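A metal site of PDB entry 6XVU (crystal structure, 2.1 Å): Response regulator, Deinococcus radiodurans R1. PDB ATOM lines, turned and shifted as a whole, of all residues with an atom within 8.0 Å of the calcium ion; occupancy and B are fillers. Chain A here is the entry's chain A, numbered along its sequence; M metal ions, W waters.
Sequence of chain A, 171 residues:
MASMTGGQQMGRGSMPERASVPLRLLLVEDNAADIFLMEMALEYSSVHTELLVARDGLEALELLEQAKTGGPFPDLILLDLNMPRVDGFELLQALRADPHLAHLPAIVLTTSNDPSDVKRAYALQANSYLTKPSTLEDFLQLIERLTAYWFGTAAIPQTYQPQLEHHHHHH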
ATOM      1  N   VAL A  28      15.567 -11.410 -24.767  1.00  0.00           N
ATOM      2  CA  VAL A  28      15.703 -12.786 -24.198  1.00  0.00           C
ATOM      3  C   VAL A  28      17.059 -12.846 -23.527  1.00  0.00           C
ATOM      4  O   VAL A  28      18.080 -12.794 -24.209  1.00  0.00           O
ATOM      5  CB  VAL A  28      15.532 -13.905 -25.229  1.00  0.00           C
ATOM      6  CG1 VAL A  28      15.323 -15.262 -24.574  1.00  0.00           C
ATOM      7  CG2 VAL A  28      14.392 -13.613 -26.211  1.00  0.00           C
ATOM      8  N   GLU A  29      17.050 -12.837 -22.220  1.00  0.00           N
ATOM      9  CA  GLU A  29      18.253 -12.640 -21.379  1.00  0.00           C
ATOM     10  C   GLU A  29      17.978 -13.237 -20.012  1.00  0.00           C
ATOM     11  O   GLU A  29      16.873 -12.988 -19.485  1.00  0.00           O
ATOM     12  CB  GLU A  29      18.539 -11.144 -21.321  1.00  0.00           C
ATOM     13  CG  GLU A  29      19.623 -10.770 -20.318  1.00  0.00           C
ATOM     14  CD  GLU A  29      20.979 -11.362 -20.634  1.00  0.00           C
ATOM     15  OE1 GLU A  29      21.580 -10.949 -21.649  1.00  0.00           O
ATOM     16  OE2 GLU A  29      21.440 -12.245 -19.840  1.00  0.00           O
ATOM     17  N   ASP A  30      18.904 -14.042 -19.486  1.00  0.00           N
ATOM     18  CA  ASP A  30      18.771 -14.727 -18.189  1.00  0.00           C
ATOM     19  C   ASP A  30      19.274 -13.832 -17.037  1.00  0.00           C
ATOM     20  O   ASP A  30      18.741 -13.938 -15.959  1.00  0.00           O
ATOM     21  CB  ASP A  30      19.477 -16.081 -18.229  1.00  0.00           C
ATOM     22  CG  ASP A  30      20.962 -16.035 -18.594  1.00  0.00           C
ATOM     23  OD1 ASP A  30      21.332 -15.215 -19.424  1.00  0.00           O
ATOM     24  OD2 ASP A  30      21.758 -16.808 -17.999  1.00  0.00           O
ATOM     25  N   ASN A  31      20.245 -12.951 -17.290  1.00  0.00           N
ATOM     26  CA  ASN A  31      20.867 -12.134 -16.230  1.00  0.00           C
ATOM     27  C   ASN A  31      20.092 -10.809 -16.034  1.00  0.00           C
ATOM     28  O   ASN A  31      19.981  -9.980 -16.967  1.00  0.00           O
ATOM     29  CB  ASN A  31      22.360 -11.951 -16.492  1.00  0.00           C
ATOM     30  CG  ASN A  31      23.003 -11.397 -15.228  1.00  0.00           C
ATOM     31  OD1 ASN A  31      22.833 -11.944 -14.127  1.00  0.00           O
ATOM     32  ND2 ASN A  31      23.699 -10.289 -15.372  1.00  0.00           N
ATOM     33  N   ASP A  34      21.707  -7.427 -17.005  1.00  0.00           N
ATOM     34  CA  ASP A  34      21.699  -7.135 -18.467  1.00  0.00           C
ATOM     35  C   ASP A  34      20.324  -6.556 -18.852  1.00  0.00           C
ATOM     36  O   ASP A  34      20.244  -5.664 -19.710  1.00  0.00           O
ATOM     37  CB  ASP A  34      22.086  -8.379 -19.250  1.00  0.00           C
ATOM     38  CG  ASP A  34      23.530  -8.865 -19.094  1.00  0.00           C
ATOM     39  OD1 ASP A  34      23.844  -9.561 -18.097  1.00  0.00           O
ATOM     40  OD2 ASP A  34      24.339  -8.564 -19.966  1.00  0.00           O
ATOM     41  N   ARG A  55      13.184 -14.727 -19.998  1.00  0.00           N
ATOM     42  CA  ARG A  55      14.418 -15.107 -19.243  1.00  0.00           C
ATOM     43  C   ARG A  55      15.143 -16.279 -19.907  1.00  0.00           C
ATOM     44  O   ARG A  55      16.261 -16.556 -19.518  1.00  0.00           O
ATOM     45  CB  ARG A  55      14.059 -15.455 -17.804  1.00  0.00           C
ATOM     46  CG  ARG A  55      13.551 -14.271 -16.972  1.00  0.00           C
ATOM     47  CD  ARG A  55      14.216 -12.916 -17.175  1.00  0.00           C
ATOM     48  NE  ARG A  55      15.471 -12.895 -16.420  1.00  0.00           N
ATOM     49  CZ  ARG A  55      15.590 -12.610 -15.104  1.00  0.00           C
ATOM     50  NH1 ARG A  55      14.553 -12.269 -14.359  1.00  0.00           N
ATOM     51  NH2 ARG A  55      16.757 -12.684 -14.513  1.00  0.00           N
ATOM     52  N   ASP A  80      20.404 -13.545 -26.118  1.00  0.00           N
ATOM     53  CA  ASP A  80      21.714 -14.023 -25.635  1.00  0.00           C
ATOM     54  C   ASP A  80      21.898 -15.482 -26.068  1.00  0.00           C
ATOM     55  O   ASP A  80      20.901 -16.096 -26.480  1.00  0.00           O
ATOM     56  CB  ASP A  80      21.721 -13.746 -24.146  1.00  0.00           C
ATOM     57  CG  ASP A  80      22.994 -14.139 -23.461  1.00  0.00           C
ATOM     58  OD1 ASP A  80      24.091 -13.764 -23.977  1.00  0.00           O
ATOM     59  OD2 ASP A  80      22.834 -14.977 -22.565  1.00  0.00           O
ATOM     60  N   LEU A  81      23.111 -15.967 -26.106  1.00  0.00           N
ATOM     61  CA  LEU A  81      23.420 -17.351 -26.575  1.00  0.00           C
ATOM     62  C   LEU A  81      23.279 -18.310 -25.393  1.00  0.00           C
ATOM     63  O   LEU A  81      22.546 -19.287 -25.498  1.00  0.00           O
ATOM     64  CB  LEU A  81      24.833 -17.390 -27.165  1.00  0.00           C
ATOM     65  CG  LEU A  81      24.984 -16.651 -28.497  1.00  0.00           C
ATOM     66  CD1 LEU A  81      26.364 -16.912 -29.086  1.00  0.00           C
ATOM     67  CD2 LEU A  81      23.867 -16.981 -29.480  1.00  0.00           C
ATOM     68  N   ASN A  82      23.953 -18.009 -24.294  1.00  0.00           N
ATOM     69  CA  ASN A  82      24.068 -18.933 -23.147  1.00  0.00           C
ATOM     70  C   ASN A  82      22.929 -18.628 -22.171  1.00  0.00           C
ATOM     71  O   ASN A  82      23.037 -17.627 -21.436  1.00  0.00           O
ATOM     72  CB  ASN A  82      25.441 -18.889 -22.491  1.00  0.00           C
ATOM     73  CG  ASN A  82      25.546 -19.986 -21.467  1.00  0.00           C
ATOM     74  OD1 ASN A  82      24.711 -20.882 -21.441  1.00  0.00           O
ATOM     75  ND2 ASN A  82      26.528 -19.904 -20.599  1.00  0.00           N
ATOM     76  N   MET A  83      21.866 -19.431 -22.216  1.00  0.00           N
ATOM     77  CA  MET A  83      20.637 -19.251 -21.400  1.00  0.00           C
ATOM     78  C   MET A  83      20.148 -20.624 -21.033  1.00  0.00           C
ATOM     79  O   MET A  83      20.287 -21.541 -21.826  1.00  0.00           O
ATOM     80  CB  MET A  83      19.511 -18.555 -22.171  1.00  0.00           C
ATOM     81  CG  MET A  83      19.886 -17.189 -22.674  1.00  0.00           C
ATOM     82  SD  MET A  83      18.458 -16.364 -23.418  1.00  0.00           S
ATOM     83  CE  MET A  83      18.293 -17.349 -24.924  1.00  0.00           C
ATOM     84  N   PRO A  84      19.558 -20.805 -19.839  1.00  0.00           N
ATOM     85  CA  PRO A  84      19.114 -22.126 -19.449  1.00  0.00           C
ATOM     86  C   PRO A  84      17.907 -22.605 -20.275  1.00  0.00           C
ATOM     87  O   PRO A  84      17.194 -21.809 -20.823  1.00  0.00           O
ATOM     88  CB  PRO A  84      18.830 -21.949 -17.935  1.00  0.00           C
ATOM     89  CG  PRO A  84      18.455 -20.510 -17.790  1.00  0.00           C
ATOM     90  CD  PRO A  84      19.264 -19.769 -18.841  1.00  0.00           C
ATOM     91  N   LEU A 109      22.595 -10.669 -29.089  1.00  0.00           N
ATOM     92  CA  LEU A 109      23.359  -9.707 -28.271  1.00  0.00           C
ATOM     93  C   LEU A 109      23.948 -10.496 -27.123  1.00  0.00           C
ATOM     94  O   LEU A 109      23.177 -10.947 -26.256  1.00  0.00           O
ATOM     95  CB  LEU A 109      22.424  -8.581 -27.799  1.00  0.00           C
ATOM     96  CG  LEU A 109      23.022  -7.617 -26.778  1.00  0.00           C
ATOM     97  CD1 LEU A 109      24.123  -6.815 -27.397  1.00  0.00           C
ATOM     98  CD2 LEU A 109      21.926  -6.739 -26.202  1.00  0.00           C
ATOM     99  N   THR A 110      25.271 -10.679 -27.131  1.00  0.00           N
ATOM    100  CA  THR A 110      25.939 -11.687 -26.301  1.00  0.00           C
ATOM    101  C   THR A 110      27.360 -11.235 -25.982  1.00  0.00           C
ATOM    102  O   THR A 110      27.923 -10.392 -26.742  1.00  0.00           O
ATOM    103  CB  THR A 110      25.846 -13.010 -27.072  1.00  0.00           C
ATOM    104  OG1 THR A 110      25.828 -14.080 -26.112  1.00  0.00           O
ATOM    105  CG2 THR A 110      26.851 -13.094 -28.224  1.00  0.00           C
ATOM    106  N   THR A 111      27.980 -11.772 -24.927  1.00  0.00           N
ATOM    107  CA  THR A 111      29.361 -11.314 -24.545  1.00  0.00           C
ATOM    108  C   THR A 111      30.421 -12.074 -25.399  1.00  0.00           C
ATOM    109  O   THR A 111      31.486 -11.505 -25.653  1.00  0.00           O
ATOM    110  CB  THR A 111      29.685 -11.451 -23.054  1.00  0.00           C
ATOM    111  OG1 THR A 111      29.548 -12.833 -22.799  1.00  0.00           O
ATOM    112  CG2 THR A 111      28.846 -10.663 -22.065  1.00  0.00           C
ATOM    113  N   LYS A 132      28.201  -7.624 -26.691  1.00  0.00           N
ATOM    114  CA  LYS A 132      28.143  -6.708 -25.516  1.00  0.00           C
ATOM    115  C   LYS A 132      29.510  -6.093 -25.294  1.00  0.00           C
ATOM    116  O   LYS A 132      30.506  -6.765 -25.178  1.00  0.00           O
ATOM    117  CB  LYS A 132      27.681  -7.464 -24.265  1.00  0.00           C
ATOM    118  CG  LYS A 132      26.222  -7.918 -24.344  1.00  0.00           C
ATOM    119  CD  LYS A 132      25.841  -8.780 -23.159  1.00  0.00           C
ATOM    120  CE  LYS A 132      24.468  -9.369 -23.257  1.00  0.00           C
ATOM    121  NZ  LYS A 132      24.260 -10.404 -22.233  1.00  0.00           N
HETATM  122 CA    CA M   1      23.462 -15.558 -20.439  1.00  0.00          CA
HETATM  123  O   HOH W   1      24.204 -17.107 -18.659  1.00  0.00           O
HETATM  124  O   HOH W   2      23.592 -13.361 -20.073  1.00  0.00           O
HETATM  125  O   HOH W   3      25.579 -15.605 -20.976  1.00  0.00           O
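OD1 of Asp 80 lies within salt-bridge range of NZ of Lys 132, at 3.8 Å.
The side-chain carboxylate (OD1) of Asp 80 lies within hydrogen-bond range of the side-chain hydroxyl (OG1) of Thr 110.
The backbone NH (N) of Asp 80 is in hydrogen-bond range of the backbone carbonyl oxygen (O) of Val 28 (3.1 Å).
The guanidinium group (NH2) of Arg 55 sits at hydrogen-bond distance from the backbone carbonyl oxygen (O) of Asp 30 (2.8 Å).
The side-chain carboxylate (OE2) of Glu 29 is in hydrogen-bond range of the backbone NH (N) of Asn 31.
The side-chain amino group of Lys 132 lies within salt-bridge range of the side-chain carboxylate of Glu 29 (2.8 Å).
The guanidinium group (NE) of Arg 55 lies close to the backbone carbonyl oxygen (O) of Glu 29 (3.4 Å).
Residues that only touch the calcium ion: Glu 29.
Four residues have an atom within 4 Å of the calcium ion: Glu 29, Asp 30, Asp 80 and Asn 82.
The calcium ion is bound by water W3 (2.2 Å).
Water W2 is bound to the calcium ion, 2.2 Å away.
OD2 of Asp 80 is bound to the calcium ion, 2.3 Å away.
The calcium ion is bound by O of Asn 82.
The side-chain carboxylate (OD1) of Asp 30 binds the calcium ion (2.4 Å).
The calcium ion is bound by water W1, 2.5 Å away.
The calcium ion has six donor atoms within binding distance.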
